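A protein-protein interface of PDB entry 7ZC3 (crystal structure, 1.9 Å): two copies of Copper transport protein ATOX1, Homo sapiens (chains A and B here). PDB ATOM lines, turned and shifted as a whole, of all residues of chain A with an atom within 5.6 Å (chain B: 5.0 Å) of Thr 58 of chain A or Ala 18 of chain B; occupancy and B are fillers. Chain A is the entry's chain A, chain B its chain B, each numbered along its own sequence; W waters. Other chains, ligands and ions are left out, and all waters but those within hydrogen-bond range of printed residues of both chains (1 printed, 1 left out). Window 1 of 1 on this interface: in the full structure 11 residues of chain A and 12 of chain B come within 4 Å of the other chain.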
ATOM      1  N   VAL A   8      14.290 -11.734 -15.106  1.00  0.00           N
ATOM      2  CA  VAL A   8      14.592 -13.120 -15.467  1.00  0.00           C
ATOM      3  C   VAL A   8      15.851 -13.526 -14.711  1.00  0.00           C
ATOM      4  O   VAL A   8      16.895 -12.888 -14.869  1.00  0.00           O
ATOM      5  CB  VAL A   8      14.811 -13.293 -16.981  1.00  0.00           C
ATOM      6  CG1 VAL A   8      15.124 -14.758 -17.286  1.00  0.00           C
ATOM      7  CG2 VAL A   8      13.599 -12.799 -17.792  1.00  0.00           C
ATOM      8  N   ALA A  18      20.527 -18.166 -23.884  1.00  0.00           N
ATOM      9  CA  ALA A  18      19.334 -18.995 -24.052  1.00  0.00           C
ATOM     10  C   ALA A  18      18.082 -18.140 -24.149  1.00  0.00           C
ATOM     11  O   ALA A  18      17.175 -18.433 -24.939  1.00  0.00           O
ATOM     12  CB  ALA A  18      19.210 -19.998 -22.908  1.00  0.00           C
ATOM     13  N   VAL A  19      18.002 -17.085 -23.338  1.00  0.00           N
ATOM     14  CA  VAL A  19      16.902 -16.130 -23.455  1.00  0.00           C
ATOM     15  C   VAL A  19      16.854 -15.553 -24.864  1.00  0.00           C
ATOM     16  O   VAL A  19      15.798 -15.509 -25.504  1.00  0.00           O
ATOM     17  CB  VAL A  19      17.047 -15.021 -22.402  1.00  0.00           C
ATOM     18  CG1 VAL A  19      16.103 -13.858 -22.731  1.00  0.00           C
ATOM     19  CG2 VAL A  19      16.756 -15.589 -21.019  1.00  0.00           C
ATOM     20  N   VAL A  22      15.324 -18.134 -27.380  1.00  0.00           N
ATOM     21  CA  VAL A  22      13.885 -18.387 -27.423  1.00  0.00           C
ATOM     22  C   VAL A  22      13.167 -17.167 -27.986  1.00  0.00           C
ATOM     23  O   VAL A  22      12.136 -17.302 -28.657  1.00  0.00           O
ATOM     24  CB  VAL A  22      13.323 -18.808 -26.047  1.00  0.00           C
ATOM     25  CG1 VAL A  22      14.134 -20.001 -25.472  1.00  0.00           C
ATOM     26  CG2 VAL A  22      13.204 -17.632 -25.080  1.00  0.00           C
ATOM     27  N   THR A  54       6.781 -17.118 -23.670  1.00  0.00           N
ATOM     28  CA  THR A  54       8.019 -17.413 -24.384  1.00  0.00           C
ATOM     29  C   THR A  54       9.208 -17.423 -23.436  1.00  0.00           C
ATOM     30  O   THR A  54      10.065 -18.314 -23.516  1.00  0.00           O
ATOM     31  CB  THR A  54       8.242 -16.393 -25.500  1.00  0.00           C
ATOM     32  OG1 THR A  54       7.186 -16.515 -26.452  1.00  0.00           O
ATOM     33  CG2 THR A  54       9.560 -16.643 -26.212  1.00  0.00           C
ATOM     34  N   LEU A  55       9.279 -16.436 -22.529  1.00  0.00           N
ATOM     35  CA  LEU A  55      10.396 -16.393 -21.585  1.00  0.00           C
ATOM     36  C   LEU A  55      10.333 -17.569 -20.622  1.00  0.00           C
ATOM     37  O   LEU A  55      11.370 -18.136 -20.259  1.00  0.00           O
ATOM     38  CB  LEU A  55      10.399 -15.062 -20.829  1.00  0.00           C
ATOM     39  CG  LEU A  55      10.719 -13.848 -21.699  1.00  0.00           C
ATOM     40  CD1 LEU A  55      10.520 -12.529 -20.950  1.00  0.00           C
ATOM     41  CD2 LEU A  55      12.164 -13.952 -22.220  1.00  0.00           C
ATOM     42  N   LYS A  56       9.127 -17.974 -20.216  1.00  0.00           N
ATOM     43  CA  LYS A  56       9.033 -19.078 -19.266  1.00  0.00           C
ATOM     44  C   LYS A  56       9.468 -20.413 -19.871  1.00  0.00           C
ATOM     45  O   LYS A  56       9.813 -21.332 -19.118  1.00  0.00           O
ATOM     46  CB  LYS A  56       7.617 -19.164 -18.696  1.00  0.00           C
ATOM     47  CG  LYS A  56       7.271 -17.953 -17.841  1.00  0.00           C
ATOM     48  CD  LYS A  56       5.878 -18.036 -17.226  1.00  0.00           C
ATOM     49  CE  LYS A  56       5.961 -18.027 -15.701  1.00  0.00           C
ATOM     50  NZ  LYS A  56       4.624 -18.112 -15.044  1.00  0.00           N
ATOM     51  N   LYS A  57       9.517 -20.535 -21.201  1.00  0.00           N
ATOM     52  CA  LYS A  57      10.063 -21.760 -21.790  1.00  0.00           C
ATOM     53  C   LYS A  57      11.538 -21.961 -21.474  1.00  0.00           C
ATOM     54  O   LYS A  57      12.050 -23.070 -21.663  1.00  0.00           O
ATOM     55  CB  LYS A  57       9.913 -21.782 -23.309  1.00  0.00           C
ATOM     56  CG  LYS A  57       8.539 -21.499 -23.853  1.00  0.00           C
ATOM     57  CD  LYS A  57       8.506 -21.919 -25.319  1.00  0.00           C
ATOM     58  CE  LYS A  57       7.101 -21.881 -25.902  1.00  0.00           C
ATOM     59  NZ  LYS A  57       7.153 -21.362 -27.302  1.00  0.00           N
ATOM     60  N   THR A  58      12.249 -20.919 -21.032  1.00  0.00           N
ATOM     61  CA  THR A  58      13.641 -21.116 -20.668  1.00  0.00           C
ATOM     62  C   THR A  58      13.774 -22.022 -19.452  1.00  0.00           C
ATOM     63  O   THR A  58      14.857 -22.565 -19.225  1.00  0.00           O
ATOM     64  CB  THR A  58      14.332 -19.795 -20.354  1.00  0.00           C
ATOM     65  OG1 THR A  58      13.613 -19.130 -19.304  1.00  0.00           O
ATOM     66  CG2 THR A  58      14.363 -18.899 -21.594  1.00  0.00           C
ATOM     67  N   GLY A  59      12.693 -22.208 -18.690  1.00  0.00           N
ATOM     68  CA  GLY A  59      12.762 -22.811 -17.374  1.00  0.00           C
ATOM     69  C   GLY A  59      13.251 -21.878 -16.292  1.00  0.00           C
ATOM     70  O   GLY A  59      13.470 -22.324 -15.155  1.00  0.00           O
ATOM     71  N   LYS A  60      13.441 -20.602 -16.606  1.00  0.00           N
ATOM     72  CA  LYS A  60      13.905 -19.640 -15.620  1.00  0.00           C
ATOM     73  C   LYS A  60      12.723 -18.966 -14.934  1.00  0.00           C
ATOM     74  O   LYS A  60      11.594 -18.970 -15.433  1.00  0.00           O
ATOM     75  CB  LYS A  60      14.808 -18.596 -16.278  1.00  0.00           C
ATOM     76  CG  LYS A  60      15.925 -19.222 -17.085  1.00  0.00           C
ATOM     77  CD  LYS A  60      17.256 -18.559 -16.794  1.00  0.00           C
ATOM     78  CE  LYS A  60      18.058 -19.366 -15.797  1.00  0.00           C
ATOM     79  NZ  LYS A  60      17.259 -19.846 -14.656  1.00  0.00           N
ATOM     80  N   VAL A  62      10.570 -15.979 -14.094  1.00  0.00           N
ATOM     81  CA  VAL A  62      10.281 -14.763 -14.850  1.00  0.00           C
ATOM     82  C   VAL A  62       9.197 -13.980 -14.124  1.00  0.00           C
ATOM     83  O   VAL A  62       8.219 -14.566 -13.649  1.00  0.00           O
ATOM     84  CB  VAL A  62       9.835 -15.116 -16.287  1.00  0.00           C
ATOM     85  CG1 VAL A  62       9.509 -13.866 -17.098  1.00  0.00           C
ATOM     86  CG2 VAL A  62      10.922 -15.972 -16.983  1.00  0.00           C
ATOM     87  N   GLY B  14      22.283 -22.394 -12.172  1.00  0.00           N
ATOM     88  CA  GLY B  14      21.011 -21.890 -12.671  1.00  0.00           C
ATOM     89  C   GLY B  14      20.607 -22.519 -13.992  1.00  0.00           C
ATOM     90  O   GLY B  14      19.411 -22.711 -14.261  1.00  0.00           O
ATOM     91  N   CYS B  15      21.587 -22.825 -14.849  1.00  0.00           N
ATOM     92  CA  CYS B  15      21.289 -23.546 -16.086  1.00  0.00           C
ATOM     93  C   CYS B  15      20.729 -24.933 -15.776  1.00  0.00           C
ATOM     94  O   CYS B  15      19.788 -25.407 -16.431  1.00  0.00           O
ATOM     95  CB  CYS B  15      22.557 -23.689 -16.933  1.00  0.00           C
ATOM     96  SG  CYS B  15      23.269 -22.212 -17.697  1.00  0.00           S
ATOM     97  N   ALA B  16      21.311 -25.605 -14.781  1.00  0.00           N
ATOM     98  CA  ALA B  16      20.805 -26.919 -14.385  1.00  0.00           C
ATOM     99  C   ALA B  16      19.402 -26.813 -13.798  1.00  0.00           C
ATOM    100  O   ALA B  16      18.535 -27.655 -14.074  1.00  0.00           O
ATOM    101  CB  ALA B  16      21.776 -27.564 -13.392  1.00  0.00           C
ATOM    102  N   GLU B  17      19.157 -25.780 -12.988  1.00  0.00           N
ATOM    103  CA  GLU B  17      17.818 -25.579 -12.444  1.00  0.00           C
ATOM    104  C   GLU B  17      16.789 -25.428 -13.560  1.00  0.00           C
ATOM    105  O   GLU B  17      15.689 -25.987 -13.478  1.00  0.00           O
ATOM    106  CB  GLU B  17      17.807 -24.351 -11.526  1.00  0.00           C
ATOM    107  CG  GLU B  17      18.562 -24.555 -10.212  1.00  0.00           C
ATOM    108  CD  GLU B  17      18.570 -23.310  -9.324  1.00  0.00           C
ATOM    109  OE1 GLU B  17      18.000 -22.264  -9.724  1.00  0.00           O
ATOM    110  OE2 GLU B  17      19.143 -23.381  -8.217  1.00  0.00           O
ATOM    111  N   ALA B  18      17.142 -24.691 -14.623  1.00  0.00           N
ATOM    112  CA  ALA B  18      16.209 -24.468 -15.726  1.00  0.00           C
ATOM    113  C   ALA B  18      15.847 -25.779 -16.417  1.00  0.00           C
ATOM    114  O   ALA B  18      14.677 -26.018 -16.741  1.00  0.00           O
ATOM    115  CB  ALA B  18      16.812 -23.485 -16.739  1.00  0.00           C
ATOM    116  N   VAL B  19      16.842 -26.635 -16.666  1.00  0.00           N
ATOM    117  CA  VAL B  19      16.564 -27.947 -17.243  1.00  0.00           C
ATOM    118  C   VAL B  19      15.647 -28.744 -16.329  1.00  0.00           C
ATOM    119  O   VAL B  19      14.689 -29.384 -16.784  1.00  0.00           O
ATOM    120  CB  VAL B  19      17.878 -28.707 -17.506  1.00  0.00           C
ATOM    121  CG1 VAL B  19      17.577 -30.169 -17.838  1.00  0.00           C
ATOM    122  CG2 VAL B  19      18.661 -28.046 -18.622  1.00  0.00           C
ATOM    123  N   SER B  20      15.931 -28.727 -15.027  1.00  0.00           N
ATOM    124  CA  SER B  20      15.082 -29.422 -14.069  1.00  0.00           C
ATOM    125  C   SER B  20      13.642 -28.924 -14.144  1.00  0.00           C
ATOM    126  O   SER B  20      12.698 -29.723 -14.167  1.00  0.00           O
ATOM    127  CB  SER B  20      15.638 -29.232 -12.656  1.00  0.00           C
ATOM    128  OG  SER B  20      14.713 -29.680 -11.678  1.00  0.00           O
ATOM    129  N   ARG B  21      13.455 -27.599 -14.174  1.00  0.00           N
ATOM    130  CA  ARG B  21      12.105 -27.035 -14.197  1.00  0.00           C
ATOM    131  C   ARG B  21      11.312 -27.473 -15.432  1.00  0.00           C
ATOM    132  O   ARG B  21      10.117 -27.792 -15.320  1.00  0.00           O
ATOM    133  CB  ARG B  21      12.175 -25.506 -14.128  1.00  0.00           C
ATOM    134  CG  ARG B  21      12.380 -24.960 -12.727  1.00  0.00           C
ATOM    135  CD  ARG B  21      11.963 -23.478 -12.626  1.00  0.00           C
ATOM    136  NE  ARG B  21      12.508 -22.858 -11.420  1.00  0.00           N
ATOM    137  CZ  ARG B  21      13.710 -22.297 -11.341  1.00  0.00           C
ATOM    138  NH1 ARG B  21      14.513 -22.212 -12.396  1.00  0.00           N
ATOM    139  NH2 ARG B  21      14.127 -21.820 -10.172  1.00  0.00           N
ATOM    140  N   VAL B  22      11.928 -27.468 -16.624  1.00  0.00           N
ATOM    141  CA  VAL B  22      11.140 -27.850 -17.802  1.00  0.00           C
ATOM    142  C   VAL B  22      10.858 -29.349 -17.793  1.00  0.00           C
ATOM    143  O   VAL B  22       9.780 -29.791 -18.229  1.00  0.00           O
ATOM    144  CB  VAL B  22      11.800 -27.402 -19.128  1.00  0.00           C
ATOM    145  CG1 VAL B  22      12.140 -25.923 -19.093  1.00  0.00           C
ATOM    146  CG2 VAL B  22      13.038 -28.236 -19.473  1.00  0.00           C
ATOM    147  N   LYS B  57      13.380 -26.508 -25.991  1.00  0.00           N
ATOM    148  CA  LYS B  57      12.499 -25.405 -25.620  1.00  0.00           C
ATOM    149  C   LYS B  57      13.228 -24.352 -24.788  1.00  0.00           C
ATOM    150  O   LYS B  57      12.909 -23.159 -24.882  1.00  0.00           O
ATOM    151  CB  LYS B  57      11.312 -25.972 -24.839  1.00  0.00           C
ATOM    152  CG  LYS B  57       9.995 -25.267 -24.996  1.00  0.00           C
ATOM    153  CD  LYS B  57       8.913 -26.102 -24.317  1.00  0.00           C
ATOM    154  CE  LYS B  57       9.387 -26.540 -22.922  1.00  0.00           C
ATOM    155  NZ  LYS B  57       9.295 -25.408 -21.937  1.00  0.00           N
ATOM    156  N   THR B  58      14.203 -24.778 -23.971  1.00  0.00           N
ATOM    157  CA  THR B  58      14.959 -23.907 -23.078  1.00  0.00           C
ATOM    158  C   THR B  58      15.813 -22.881 -23.804  1.00  0.00           C
ATOM    159  O   THR B  58      16.304 -21.947 -23.156  1.00  0.00           O
ATOM    160  CB  THR B  58      15.898 -24.718 -22.193  1.00  0.00           C
ATOM    161  OG1 THR B  58      16.915 -25.321 -23.017  1.00  0.00           O
ATOM    162  CG2 THR B  58      15.132 -25.795 -21.420  1.00  0.00           C
ATOM    163  N   LYS B  60      18.699 -23.726 -24.988  1.00  0.00           N
ATOM    164  CA  LYS B  60      20.066 -24.221 -24.884  1.00  0.00           C
ATOM    165  C   LYS B  60      20.390 -25.122 -26.077  1.00  0.00           C
ATOM    166  O   LYS B  60      19.504 -25.593 -26.792  1.00  0.00           O
ATOM    167  CB  LYS B  60      20.277 -24.980 -23.573  1.00  0.00           C
ATOM    168  CG  LYS B  60      19.982 -24.126 -22.331  1.00  0.00           C
ATOM    169  CD  LYS B  60      20.183 -24.903 -21.028  1.00  0.00           C
ATOM    170  CE  LYS B  60      19.505 -24.215 -19.821  1.00  0.00           C
ATOM    171  NZ  LYS B  60      19.762 -22.734 -19.779  1.00  0.00           N
HETATM  172  O   HOH W   1      17.230 -21.806 -20.592  1.00  0.00           O
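Ala 18 of chain A touches Thr 58 of chain B, and with the chains exchanged Thr 58 of chain A touches Ala 18 of chain B. Lys 57 of chain B touches its own counterpart, Lys 57 of chain A. Lys 57 of chain A touches Thr 58 of chain B, but with the chains exchanged Thr 58 of chain A does not touch Lys 57 of chain B (4.5 Å). Thr 58 of chain A touches its own counterpart, Thr 58 of chain B. Of the 12 pairs that touch across the chains among the printed residues, 6 have their exchanged pair printed and touching as well.
The side-chain hydroxyl (OG1) of Thr 58 of chain A lies within hydrogen-bond range of the backbone carbonyl oxygen (O) of Leu 55 of chain A. The side-chain hydroxyl (OG1) of Thr 58 of chain A is in hydrogen-bond range of the backbone NH (N) of Lys 60 of chain A (3.1 Å). OE1 of Glu 17 of chain B is in salt-bridge range of NH2 of Arg 21 of chain B (3.9 Å). OG1 of Thr 58 of chain B is in hydrogen-bond range of N of Lys 60 of chain B, 3.1 Å away.
Water W1 lies within hydrogen-bond range of the backbone carbonyl oxygen (O) of Thr 58 of chain B (2.7 Å), the side-chain amino group (NZ) of Lys 60 of chain B (2.8 Å) and the backbone carbonyl oxygen (O) of Thr 58 of chain A (2.8 Å).
NH1 of Arg 21 of chain B lies within hydrogen-bond range of O of Gly 59 of chain A, at 3.0 Å. The backbone carbonyl oxygen (O) of Lys 57 of chain B lies close to the backbone carbonyl oxygen (O) of Lys 57 of chain A (3.3 Å).
Of the printed residues of chain B, Val 22 of chain A touches Lys 57 and Thr 58. Of the printed residues of chain B, Lys 57 of chain A touches Val 22 (3.8 Å), Lys 57 (3.3 Å) and Thr 58 (3.3 Å). Thr 58 of chain A touches just these residues of chain B: Ala 18 and Thr 58. Printed residues of chain B within 4 Å of Lys 60 of chain A: Gly 14 (3.6 Å). Of the printed residues of chain A, Ala 18 of chain B touches Thr 58 (3.3 Å) and Gly 59 (3.5 Å). Printed residues of chain A within 4 Å of Arg 21 of chain B: Gly 59 (3.0 Å). The nearest printed residue of chain A that does not touch Ala 18 of chain B is Lys 60 of chain A (4.2 Å).
Of the 12 printed residues of chain A, 6 touch a printed residue of chain B. Hydrophobic or aromatic side chains of chain A within 4 Å of the printed part of chain B: Ala 18 and Val 22. Printed residues of chain B that touch a printed residue of chain A: Gly 14, Ala 18, Arg 21, Val 22, Lys 57 and Thr 58. Hydrophobic or aromatic side chains of chain B that line the printed part of chain A: Ala 18 and Val 22. Among the printed residues, 12 pairs touch across the chains. Among the printed residues, no Asp or Glu carboxylate lies within 4 Å of a Lys or Arg side-chain nitrogen of the other chain.
Among the printed residues, merely in contact across the chains: Thr 58 of chain A with Ala 18 of chain B, Lys 57 of chain A with Thr 58 of chain B, Val 22 of chain A with Lys 57 of chain B, Ala 18 of chain A with Thr 58 of chain B, Gly 59 of chain A with Ala 18 of chain B, Lys 60 of chain A with Gly 14 of chain B, Gly 59 of chain A with Val 22 of chain B, Val 22 of chain A with Thr 58 of chain B, Thr 58 of chain A with Thr 58 of chain B and Lys 57 of chain A with Val 22 of chain B.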
